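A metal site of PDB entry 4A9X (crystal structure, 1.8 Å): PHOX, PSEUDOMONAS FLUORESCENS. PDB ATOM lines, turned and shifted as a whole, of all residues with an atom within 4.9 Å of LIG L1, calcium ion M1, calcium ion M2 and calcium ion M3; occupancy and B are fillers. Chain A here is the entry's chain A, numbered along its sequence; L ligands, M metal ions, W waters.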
ATOM      1  N   ASP A  69      -9.166 -19.946 -34.477  1.00  0.00           N
ATOM      2  CA  ASP A  69      -7.995 -20.078 -33.623  1.00  0.00           C
ATOM      3  C   ASP A  69      -7.186 -21.319 -34.029  1.00  0.00           C
ATOM      4  O   ASP A  69      -6.716 -21.377 -35.169  1.00  0.00           O
ATOM      5  CB  ASP A  69      -8.510 -20.023 -32.161  1.00  0.00           C
ATOM      6  CG  ASP A  69      -7.549 -19.583 -31.065  1.00  0.00           C
ATOM      7  OD1 ASP A  69      -6.348 -19.838 -31.178  1.00  0.00           O
ATOM      8  OD2 ASP A  69      -8.025 -19.086 -30.029  1.00  0.00           O
ATOM      9  N   GLU A  90     -13.144 -19.789 -31.263  1.00  0.00           N
ATOM     10  CA  GLU A  90     -13.036 -19.557 -29.827  1.00  0.00           C
ATOM     11  C   GLU A  90     -14.131 -18.760 -29.195  1.00  0.00           C
ATOM     12  O   GLU A  90     -14.721 -19.185 -28.205  1.00  0.00           O
ATOM     13  CB  GLU A  90     -11.661 -18.943 -29.475  1.00  0.00           C
ATOM     14  CG  GLU A  90     -11.351 -18.888 -27.986  1.00  0.00           C
ATOM     15  CD  GLU A  90      -9.975 -18.307 -27.710  1.00  0.00           C
ATOM     16  OE1 GLU A  90      -9.636 -17.279 -28.339  1.00  0.00           O
ATOM     17  OE2 GLU A  90      -9.226 -18.927 -26.934  1.00  0.00           O
ATOM     18  N   CYS A 179      -9.976 -23.111 -28.062  1.00  0.00           N
ATOM     19  CA  CYS A 179      -8.759 -22.334 -28.203  1.00  0.00           C
ATOM     20  C   CYS A 179      -7.855 -23.014 -29.239  1.00  0.00           C
ATOM     21  O   CYS A 179      -8.060 -22.748 -30.429  1.00  0.00           O
ATOM     22  CB  CYS A 179      -8.108 -22.173 -26.833  1.00  0.00           C
ATOM     23  SG  CYS A 179      -6.547 -21.289 -26.849  1.00  0.00           S
ATOM     24  N   GLU A 194     -10.857 -23.828 -23.387  1.00  0.00           N
ATOM     25  CA  GLU A 194     -10.016 -22.996 -22.568  1.00  0.00           C
ATOM     26  C   GLU A 194     -10.798 -22.149 -21.544  1.00  0.00           C
ATOM     27  O   GLU A 194     -11.024 -22.641 -20.455  1.00  0.00           O
ATOM     28  CB  GLU A 194      -9.109 -22.158 -23.449  1.00  0.00           C
ATOM     29  CG  GLU A 194      -7.965 -21.394 -22.747  1.00  0.00           C
ATOM     30  CD  GLU A 194      -7.388 -20.220 -23.525  1.00  0.00           C
ATOM     31  OE1 GLU A 194      -8.091 -19.716 -24.418  1.00  0.00           O
ATOM     32  OE2 GLU A 194      -6.242 -19.811 -23.245  1.00  0.00           O
ATOM     33  N   ASN A 195     -11.222 -20.912 -21.883  1.00  0.00           N
ATOM     34  CA  ASN A 195     -11.934 -20.034 -20.932  1.00  0.00           C
ATOM     35  C   ASN A 195     -13.462 -20.250 -20.905  1.00  0.00           C
ATOM     36  O   ASN A 195     -14.244 -19.300 -20.886  1.00  0.00           O
ATOM     37  CB  ASN A 195     -11.560 -18.587 -21.185  1.00  0.00           C
ATOM     38  CG  ASN A 195     -10.125 -18.282 -20.840  1.00  0.00           C
ATOM     39  OD1 ASN A 195      -9.738 -18.328 -19.674  1.00  0.00           O
ATOM     40  ND2 ASN A 195      -9.303 -17.907 -21.809  1.00  0.00           N
ATOM     41  N   ARG A 223     -18.034 -13.417 -17.080  1.00  0.00           N
ATOM     42  CA  ARG A 223     -16.944 -12.511 -17.463  1.00  0.00           C
ATOM     43  C   ARG A 223     -17.371 -11.749 -18.720  1.00  0.00           C
ATOM     44  O   ARG A 223     -16.777 -11.895 -19.792  1.00  0.00           O
ATOM     45  CB  ARG A 223     -15.623 -13.284 -17.621  1.00  0.00           C
ATOM     46  CG  ARG A 223     -14.389 -12.400 -17.625  1.00  0.00           C
ATOM     47  CD  ARG A 223     -13.097 -13.191 -17.547  1.00  0.00           C
ATOM     48  NE  ARG A 223     -12.891 -13.783 -16.222  1.00  0.00           N
ATOM     49  CZ  ARG A 223     -11.917 -14.635 -15.902  1.00  0.00           C
ATOM     50  NH1 ARG A 223     -11.026 -15.007 -16.820  1.00  0.00           N
ATOM     51  NH2 ARG A 223     -11.811 -15.108 -14.670  1.00  0.00           N
ATOM     52  N   GLU A 273      -5.349 -25.033 -23.468  1.00  0.00           N
ATOM     53  CA  GLU A 273      -4.912 -24.225 -24.589  1.00  0.00           C
ATOM     54  C   GLU A 273      -4.765 -25.170 -25.813  1.00  0.00           C
ATOM     55  O   GLU A 273      -5.617 -25.112 -26.661  1.00  0.00           O
ATOM     56  CB  GLU A 273      -3.602 -23.516 -24.279  1.00  0.00           C
ATOM     57  CG  GLU A 273      -3.103 -22.698 -25.451  1.00  0.00           C
ATOM     58  CD  GLU A 273      -3.500 -21.242 -25.428  1.00  0.00           C
ATOM     59  OE1 GLU A 273      -3.775 -20.703 -24.335  1.00  0.00           O
ATOM     60  OE2 GLU A 273      -3.447 -20.611 -26.503  1.00  0.00           O
ATOM     61  N   ASP A 292      -3.927 -22.448 -19.422  1.00  0.00           N
ATOM     62  CA  ASP A 292      -3.602 -21.032 -19.603  1.00  0.00           C
ATOM     63  C   ASP A 292      -4.312 -20.135 -18.610  1.00  0.00           C
ATOM     64  O   ASP A 292      -5.416 -19.640 -18.837  1.00  0.00           O
ATOM     65  CB  ASP A 292      -3.852 -20.553 -21.041  1.00  0.00           C
ATOM     66  CG  ASP A 292      -3.529 -19.076 -21.224  1.00  0.00           C
ATOM     67  OD1 ASP A 292      -2.848 -18.512 -20.345  1.00  0.00           O
ATOM     68  OD2 ASP A 292      -3.964 -18.492 -22.222  1.00  0.00           O
ATOM     69  N   GLU A 293      -3.640 -19.929 -17.492  1.00  0.00           N
ATOM     70  CA  GLU A 293      -4.065 -18.997 -16.451  1.00  0.00           C
ATOM     71  C   GLU A 293      -2.831 -18.715 -15.600  1.00  0.00           C
ATOM     72  O   GLU A 293      -2.004 -19.612 -15.372  1.00  0.00           O
ATOM     73  CB  GLU A 293      -5.260 -19.548 -15.647  1.00  0.00           C
ATOM     74  CG  GLU A 293      -5.684 -18.686 -14.468  1.00  0.00           C
ATOM     75  CD  GLU A 293      -7.036 -18.979 -13.839  1.00  0.00           C
ATOM     76  OE1 GLU A 293      -7.823 -19.747 -14.427  1.00  0.00           O
ATOM     77  OE2 GLU A 293      -7.299 -18.469 -12.718  1.00  0.00           O
ATOM     78  N   ARG A 294      -2.694 -17.460 -15.161  1.00  0.00           N
ATOM     79  CA  ARG A 294      -1.562 -17.033 -14.321  1.00  0.00           C
ATOM     80  C   ARG A 294      -1.376 -17.980 -13.127  1.00  0.00           C
ATOM     81  O   ARG A 294      -2.307 -18.218 -12.389  1.00  0.00           O
ATOM     82  CB  ARG A 294      -1.797 -15.606 -13.797  1.00  0.00           C
ATOM     83  CG  ARG A 294      -1.544 -14.522 -14.827  1.00  0.00           C
ATOM     84  CD  ARG A 294      -1.747 -13.151 -14.211  1.00  0.00           C
ATOM     85  NE  ARG A 294      -3.171 -12.851 -13.961  1.00  0.00           N
ATOM     86  CZ  ARG A 294      -4.004 -12.248 -14.810  1.00  0.00           C
ATOM     87  NH1 ARG A 294      -3.573 -11.857 -16.009  1.00  0.00           N
ATOM     88  NH2 ARG A 294      -5.266 -12.029 -14.467  1.00  0.00           N
ATOM     89  N   ARG A 385       1.532 -18.513 -17.423  1.00  0.00           N
ATOM     90  CA  ARG A 385       0.527 -18.727 -18.460  1.00  0.00           C
ATOM     91  C   ARG A 385       0.985 -19.651 -19.587  1.00  0.00           C
ATOM     92  O   ARG A 385       1.273 -19.196 -20.691  1.00  0.00           O
ATOM     93  CB  ARG A 385       0.032 -17.405 -19.032  1.00  0.00           C
ATOM     94  CG  ARG A 385      -0.830 -16.608 -18.072  1.00  0.00           C
ATOM     95  CD  ARG A 385      -1.463 -15.425 -18.744  1.00  0.00           C
ATOM     96  NE  ARG A 385      -2.311 -15.838 -19.838  1.00  0.00           N
ATOM     97  CZ  ARG A 385      -2.712 -15.055 -20.840  1.00  0.00           C
ATOM     98  NH1 ARG A 385      -2.299 -13.792 -20.907  1.00  0.00           N
ATOM     99  NH2 ARG A 385      -3.500 -15.537 -21.794  1.00  0.00           N
ATOM    100  N   GLU A 387       0.811 -21.459 -22.783  1.00  0.00           N
ATOM    101  CA  GLU A 387      -0.100 -21.438 -23.923  1.00  0.00           C
ATOM    102  C   GLU A 387       0.231 -22.620 -24.848  1.00  0.00           C
ATOM    103  O   GLU A 387       0.031 -23.737 -24.380  1.00  0.00           O
ATOM    104  CB  GLU A 387      -0.211 -20.056 -24.609  1.00  0.00           C
ATOM    105  CG  GLU A 387      -0.938 -19.049 -23.719  1.00  0.00           C
ATOM    106  CD  GLU A 387      -1.617 -17.884 -24.430  1.00  0.00           C
ATOM    107  OE1 GLU A 387      -2.846 -17.903 -24.635  1.00  0.00           O
ATOM    108  OE2 GLU A 387      -0.883 -16.929 -24.774  1.00  0.00           O
ATOM    109  N   TRP A 388       0.701 -22.437 -26.101  1.00  0.00           N
ATOM    110  CA  TRP A 388       0.887 -23.600 -26.954  1.00  0.00           C
ATOM    111  C   TRP A 388       2.130 -24.392 -26.667  1.00  0.00           C
ATOM    112  O   TRP A 388       3.180 -23.845 -26.324  1.00  0.00           O
ATOM    113  CB  TRP A 388       0.895 -23.246 -28.434  1.00  0.00           C
ATOM    114  CG  TRP A 388      -0.403 -22.750 -29.004  1.00  0.00           C
ATOM    115  CD1 TRP A 388      -1.242 -21.847 -28.445  1.00  0.00           C
ATOM    116  CD2 TRP A 388      -0.843 -22.915 -30.360  1.00  0.00           C
ATOM    117  NE1 TRP A 388      -2.232 -21.508 -29.341  1.00  0.00           N
ATOM    118  CE2 TRP A 388      -1.942 -22.061 -30.549  1.00  0.00           C
ATOM    119  CE3 TRP A 388      -0.372 -23.665 -31.443  1.00  0.00           C
ATOM    120  CZ2 TRP A 388      -2.648 -22.006 -31.773  1.00  0.00           C
ATOM    121  CZ3 TRP A 388      -1.027 -23.561 -32.668  1.00  0.00           C
ATOM    122  CH2 TRP A 388      -2.191 -22.800 -32.798  1.00  0.00           C
ATOM    123  N   THR A 403       3.149 -16.931 -21.939  1.00  0.00           N
ATOM    124  CA  THR A 403       2.822 -15.695 -22.635  1.00  0.00           C
ATOM    125  C   THR A 403       3.117 -14.444 -21.857  1.00  0.00           C
ATOM    126  O   THR A 403       3.621 -13.481 -22.421  1.00  0.00           O
ATOM    127  CB  THR A 403       1.407 -15.736 -23.228  1.00  0.00           C
ATOM    128  OG1 THR A 403       1.358 -14.874 -24.352  1.00  0.00           O
ATOM    129  CG2 THR A 403       0.290 -15.352 -22.232  1.00  0.00           C
ATOM    130  N   ASP A 479       2.361 -16.810 -28.133  1.00  0.00           N
ATOM    131  CA  ASP A 479       1.215 -17.649 -27.777  1.00  0.00           C
ATOM    132  C   ASP A 479       1.235 -18.939 -28.617  1.00  0.00           C
ATOM    133  O   ASP A 479       1.541 -20.007 -28.079  1.00  0.00           O
ATOM    134  CB  ASP A 479      -0.031 -16.771 -27.954  1.00  0.00           C
ATOM    135  CG  ASP A 479      -1.413 -17.349 -27.692  1.00  0.00           C
ATOM    136  OD1 ASP A 479      -1.541 -18.581 -27.678  1.00  0.00           O
ATOM    137  OD2 ASP A 479      -2.336 -16.558 -27.423  1.00  0.00           O
ATOM    138  N   ASP A 494       0.293 -12.814 -29.447  1.00  0.00           N
ATOM    139  CA  ASP A 494      -0.983 -12.325 -28.985  1.00  0.00           C
ATOM    140  C   ASP A 494      -0.693 -11.396 -27.824  1.00  0.00           C
ATOM    141  O   ASP A 494      -0.925 -11.739 -26.657  1.00  0.00           O
ATOM    142  CB  ASP A 494      -1.878 -13.467 -28.543  1.00  0.00           C
ATOM    143  CG  ASP A 494      -3.101 -12.959 -27.814  1.00  0.00           C
ATOM    144  OD1 ASP A 494      -3.479 -11.769 -28.034  1.00  0.00           O
ATOM    145  OD2 ASP A 494      -3.650 -13.730 -27.005  1.00  0.00           O
ATOM    146  N   GLU A 532      -4.954 -10.734 -33.408  1.00  0.00           N
ATOM    147  CA  GLU A 532      -3.889 -11.564 -32.895  1.00  0.00           C
ATOM    148  C   GLU A 532      -3.658 -12.623 -33.989  1.00  0.00           C
ATOM    149  O   GLU A 532      -4.550 -12.885 -34.808  1.00  0.00           O
ATOM    150  CB  GLU A 532      -4.186 -12.159 -31.517  1.00  0.00           C
ATOM    151  CG  GLU A 532      -4.952 -13.468 -31.514  1.00  0.00           C
ATOM    152  CD  GLU A 532      -5.339 -13.939 -30.125  1.00  0.00           C
ATOM    153  OE1 GLU A 532      -6.007 -13.147 -29.428  1.00  0.00           O
ATOM    154  OE2 GLU A 532      -4.913 -15.052 -29.724  1.00  0.00           O
ATOM    155  N   THR A 534      -2.950 -16.367 -34.776  1.00  0.00           N
ATOM    156  CA  THR A 534      -3.124 -17.676 -34.148  1.00  0.00           C
ATOM    157  C   THR A 534      -3.552 -18.699 -35.154  1.00  0.00           C
ATOM    158  O   THR A 534      -4.125 -18.349 -36.178  1.00  0.00           O
ATOM    159  CB  THR A 534      -4.091 -17.518 -32.968  1.00  0.00           C
ATOM    160  OG1 THR A 534      -4.189 -18.748 -32.253  1.00  0.00           O
ATOM    161  CG2 THR A 534      -5.456 -16.982 -33.406  1.00  0.00           C
ATOM    162  N   GLN A 550      -7.226 -13.509 -35.987  1.00  0.00           N
ATOM    163  CA  GLN A 550      -8.350 -13.517 -35.088  1.00  0.00           C
ATOM    164  C   GLN A 550      -8.663 -12.128 -34.581  1.00  0.00           C
ATOM    165  O   GLN A 550      -7.741 -11.340 -34.305  1.00  0.00           O
ATOM    166  CB  GLN A 550      -8.002 -14.441 -33.910  1.00  0.00           C
ATOM    167  CG  GLN A 550      -9.194 -14.807 -33.063  1.00  0.00           C
ATOM    168  CD  GLN A 550      -8.801 -15.422 -31.765  1.00  0.00           C
ATOM    169  OE1 GLN A 550      -8.042 -14.858 -30.999  1.00  0.00           O
ATOM    170  NE2 GLN A 550      -9.325 -16.604 -31.466  1.00  0.00           N
ATOM    171  N   HIS A 551      -9.966 -11.826 -34.505  1.00  0.00           N
ATOM    172  CA  HIS A 551     -10.594 -10.574 -34.032  1.00  0.00           C
ATOM    173  C   HIS A 551      -9.966  -9.289 -34.571  1.00  0.00           C
ATOM    174  O   HIS A 551      -9.639  -8.357 -33.828  1.00  0.00           O
ATOM    175  CB  HIS A 551     -10.766 -10.514 -32.496  1.00  0.00           C
ATOM    176  CG  HIS A 551      -9.498 -10.649 -31.708  1.00  0.00           C
ATOM    177  ND1 HIS A 551      -8.563  -9.640 -31.685  1.00  0.00           N
ATOM    178  CD2 HIS A 551      -9.009 -11.704 -31.020  1.00  0.00           C
ATOM    179  CE1 HIS A 551      -7.563 -10.087 -30.944  1.00  0.00           C
ATOM    180  NE2 HIS A 551      -7.781 -11.322 -30.530  1.00  0.00           N
HETATM  181  P1  LIG L   1      -6.249 -16.130 -24.754  1.00  0.00           P
HETATM  182  O1  LIG L   1      -5.284 -15.764 -25.831  1.00  0.00           O
HETATM  183  O2  LIG L   1      -7.520 -16.808 -25.316  1.00  0.00           O
HETATM  184  O3  LIG L   1      -5.600 -17.039 -23.683  1.00  0.00           O
HETATM  185  P2  LIG L   1      -5.665 -13.499 -23.943  1.00  0.00           P
HETATM  186  O4  LIG L   1      -4.195 -13.918 -23.858  1.00  0.00           O
HETATM  187  O5  LIG L   1      -6.054 -12.372 -24.960  1.00  0.00           O
HETATM  188  C1  LIG L   1      -6.776 -14.757 -23.881  1.00  0.00           C
HETATM  189  P3  LIG L   1      -6.626 -11.447 -22.061  1.00  0.00           P
HETATM  190  O6  LIG L   1      -8.060 -11.594 -22.399  1.00  0.00           O
HETATM  191  O7  LIG L   1      -5.947 -10.114 -22.310  1.00  0.00           O
HETATM  192  O8  LIG L   1      -5.662 -12.608 -22.623  1.00  0.00           O
HETATM  193  O9  LIG L   1      -6.352 -11.523 -20.416  1.00  0.00           O
HETATM  194  C2  LIG L   1      -5.116 -11.939 -19.792  1.00  0.00           C
HETATM  195  C3  LIG L   1      -5.340 -13.166 -18.947  1.00  0.00           C
HETATM  196  O10 LIG L   1      -6.172 -12.829 -17.812  1.00  0.00           O
HETATM  197  C4  LIG L   1      -6.001 -14.379 -19.599  1.00  0.00           C
HETATM  198  O11 LIG L   1      -5.501 -15.583 -19.005  1.00  0.00           O
HETATM  199  C5  LIG L   1      -7.470 -14.195 -19.255  1.00  0.00           C
HETATM  200  O12 LIG L   1      -8.166 -15.434 -19.227  1.00  0.00           O
HETATM  201  C6  LIG L   1      -7.376 -13.578 -17.846  1.00  0.00           C
HETATM  202  N1  LIG L   1      -8.463 -12.677 -17.488  1.00  0.00           N
HETATM  203  C7  LIG L   1      -9.114 -11.797 -18.303  1.00  0.00           C
HETATM  204  N2  LIG L   1     -10.030 -11.072 -17.698  1.00  0.00           N
HETATM  205  C8  LIG L   1      -9.965 -11.513 -16.376  1.00  0.00           C
HETATM  206  C9  LIG L   1     -10.689 -11.149 -15.222  1.00  0.00           C
HETATM  207  N3  LIG L   1     -11.725 -10.314 -15.224  1.00  0.00           N
HETATM  208  N4  LIG L   1     -10.371 -11.773 -14.066  1.00  0.00           N
HETATM  209  C10 LIG L   1      -9.424 -12.717 -14.076  1.00  0.00           C
HETATM  210  N5  LIG L   1      -8.686 -13.153 -15.111  1.00  0.00           N
HETATM  211  C11 LIG L   1      -9.001 -12.502 -16.232  1.00  0.00           C
HETATM  212 FE1  LG2 L   2      -7.259 -18.980 -26.209  1.00  0.00          FE
HETATM  213 FE2  LG2 L   2      -4.668 -18.917 -24.059  1.00  0.00          FE
HETATM  214  O1  LG2 L   2      -5.385 -18.721 -25.818  1.00  0.00           O
HETATM  215 CA    CA M   1      -2.997 -15.383 -25.537  1.00  0.00          CA
HETATM  216 CA    CA M   2      -3.921 -18.489 -27.433  1.00  0.00          CA
HETATM  217 CA    CA M   3      -6.030 -13.885 -27.221  1.00  0.00          CA
HETATM  218  O   HOH W   1     -10.042 -16.973 -24.557  1.00  0.00           O
HETATM  219  O   HOH W   2      -9.258 -12.081 -24.796  1.00  0.00           O
HETATM  220  O   HOH W   3      -3.963 -17.510 -29.852  1.00  0.00           O
HETATM  221  O   HOH W   4      -6.360 -17.137 -20.975  1.00  0.00           O
HETATM  222  O   HOH W   5      -8.047 -12.526 -27.055  1.00  0.00           O
HETATM  223  O   HOH W   6      -6.885 -15.137 -14.716  1.00  0.00           O
HETATM  224  O   HOH W   7      -2.118 -11.801 -23.180  1.00  0.00           O
HETATM  225  O   HOH W   8      -5.902 -11.411 -27.285  1.00  0.00           O
HETATM  226  O   HOH W   9      -7.720 -17.992 -18.272  1.00  0.00           O
HETATM  227  O   HOH W  10      -4.755 -20.435 -29.320  1.00  0.00           O
HETATM  228  O   HOH W  11      -7.689 -15.493 -28.298  1.00  0.00           O
HETATM  229  O   HOH W  12      -6.578 -18.145 -28.216  1.00  0.00           O
HETATM  230  O   HOH W  13      -1.019 -13.923 -25.004  1.00  0.00           O
HETATM  231  O   HOH W  14     -10.884 -14.644 -19.587  1.00  0.00           O
HETATM  232  O   HOH W  15      -4.690 -15.518 -16.343  1.00  0.00           O
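O11 of LIG L1 sits at hydrogen-bond distance from NE of Arg 385 (3.3 Å).
N5 of LIG L1 lies close to NH1 of Arg 223.
An oxygen (O10) of LIG L1 lies within hydrogen-bond range of the guanidinium group (NH1) of Arg 294 (3.3 Å).
O12 of LIG L1 is in hydrogen-bond range of OD1 of Asn 195 (3.3 Å).
OE1 of Glu 273 binds FE2 of LG2 L2, at 2.0 Å.
FE2 of LG2 L2 is bound by OD2 of Asp 292, 2.0 Å away.
OE1 of Glu 387 is bound to FE2 of LG2 L2 (2.2 Å).
OE2 of Glu 194 is bound to FE2 of LG2 L2.
FE1 of LG2 L2 is bound by OE2 of Glu 90.
The side-chain sulfur (SG) of Cys 179 is bound to an iron atom (FE1) of LG2 L2, 2.5 Å away.
An oxygen (O3) of LIG L1 binds an iron atom (FE2) of LG2 L2.
N of Trp 388 lies within hydrogen-bond range of O of Asp 479, at 3.2 Å.
The backbone carbonyl oxygen of Glu 532 lies within hydrogen-bond range of the backbone NH of Gln 550, at 3.0 Å.
OE1 of Glu 532 sits close to NE2 of His 551, at 2.8 Å.
The side-chain carboxylate (OE2) of Glu 273 lies close to the indole nitrogen (NE1) of Trp 388, 3.2 Å away.
The side-chain carboxylate (OE1) of Glu 387 lies close to the guanidinium group (NH2) of Arg 385, 3.8 Å away.
The side-chain carboxylate of Glu 387 sits close to the side-chain hydroxyl of Thr 403.
OE1 of Glu 194 sits close to ND2 of Asn 195 (3.4 Å).
NE2 of Gln 550 lies within hydrogen-bond range of OE1 of Glu 90.
O2 of LIG L1 lies close to OE2 of Glu 90, at 3.2 Å.
An oxygen (O3) of LIG L1 lies close to the side-chain carboxylate (OE2) of Glu 194, 2.9 Å away.
O3 of LIG L1 lies close to OD2 of Asp 292 (2.6 Å).
Of the 20 residues printed, 11 come within 4 Å of LIG L1.
The nearest printed residue that does not touch LIG L1 is Glu 273 (4.1 Å).
Residues that only touch calcium ion M1: Arg 385 (3.8 Å).
Of the 20 residues printed, 4 come within 4 Å of calcium ion M1.
Merely in contact with calcium ion M2: Cys 179 (3.9 Å) and Trp 388 (3.95 Å).
Within 4 Å of calcium ion M2: Cys 179, Glu 273, Glu 387, Trp 388 and Asp 479.
Of the 20 residues printed, 2 come within 4 Å of calcium ion M3.
OD2 of Asp 494 binds calcium ion M1 (2.3 Å).
OD2 of Asp 479 is bound to calcium ion M1 (2.3 Å).
O1 of LIG L1 is bound to calcium ion M1 (2.3 Å).
Water W13 binds calcium ion M1 (2.5 Å).
An oxygen (O4) of LIG L1 is bound to calcium ion M1, 2.5 Å away.
OE1 of Glu 387 binds calcium ion M1 (2.7 Å).
Calcium ion M1 is bound by the side-chain carboxylate (OE2) of Glu 387 (2.7 Å).
Calcium ion M1 has seven donor atoms within binding distance.
Calcium ion M2 is bound by an oxygen (O1) of LG2 L2, the side-chain carboxylate (OE2) of Glu 273, the side-chain carboxylate (OD1) of Asp 479, the side-chain carboxylate (OD2) of Asp 479, water W3, water W12 and water W10.
Calcium ion M2 has seven donor atoms within binding distance.
Slightly farther from calcium ion M2 lies the side-chain carboxylate (OE1) of Glu 387 (3.1 Å).
Calcium ion M3 is bound by OE1 of Glu 532 (2.3 Å), OD2 of Asp 494 (2.4 Å), water W5 (2.4 Å), O1 of LIG L1 (2.5 Å), water W8 (2.5 Å), water W11 (2.5 Å) and O5 of LIG L1 (2.7 Å).
Slightly farther from calcium ion M3 lies the side-chain carboxylate (OE2) of Glu 532 (3.0 Å).
Water W3 bridges the side-chain carboxylate of Glu 532 and the side-chain hydroxyl of Thr 534.
Water W12 bridges OD2 of Asp 69 (2.5 Å) and OE1 of Glu 90 (3.2 Å).
Water W4 lies within hydrogen-bond range of O11 of LIG L1 (2.7 Å), ND2 of Asn 195 (3.2 Å), NH2 of Arg 385 (3.4 Å) and O of Asp 292 (3.4 Å).
Water W9 lies within hydrogen-bond range of the side-chain amide oxygen of Asn 195 (2.5 Å), an oxygen (O12) of LIG L1 (2.8 Å) and the backbone carbonyl oxygen of Asp 292 (2.9 Å).
Water W15 bridges an oxygen (O11) of LIG L1 and the backbone NH (N) of Arg 294.
Water W14 lies within hydrogen-bond range of the guanidinium group of Arg 223 (2.8 Å) and an oxygen (O12) of LIG L1 (2.9 Å).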
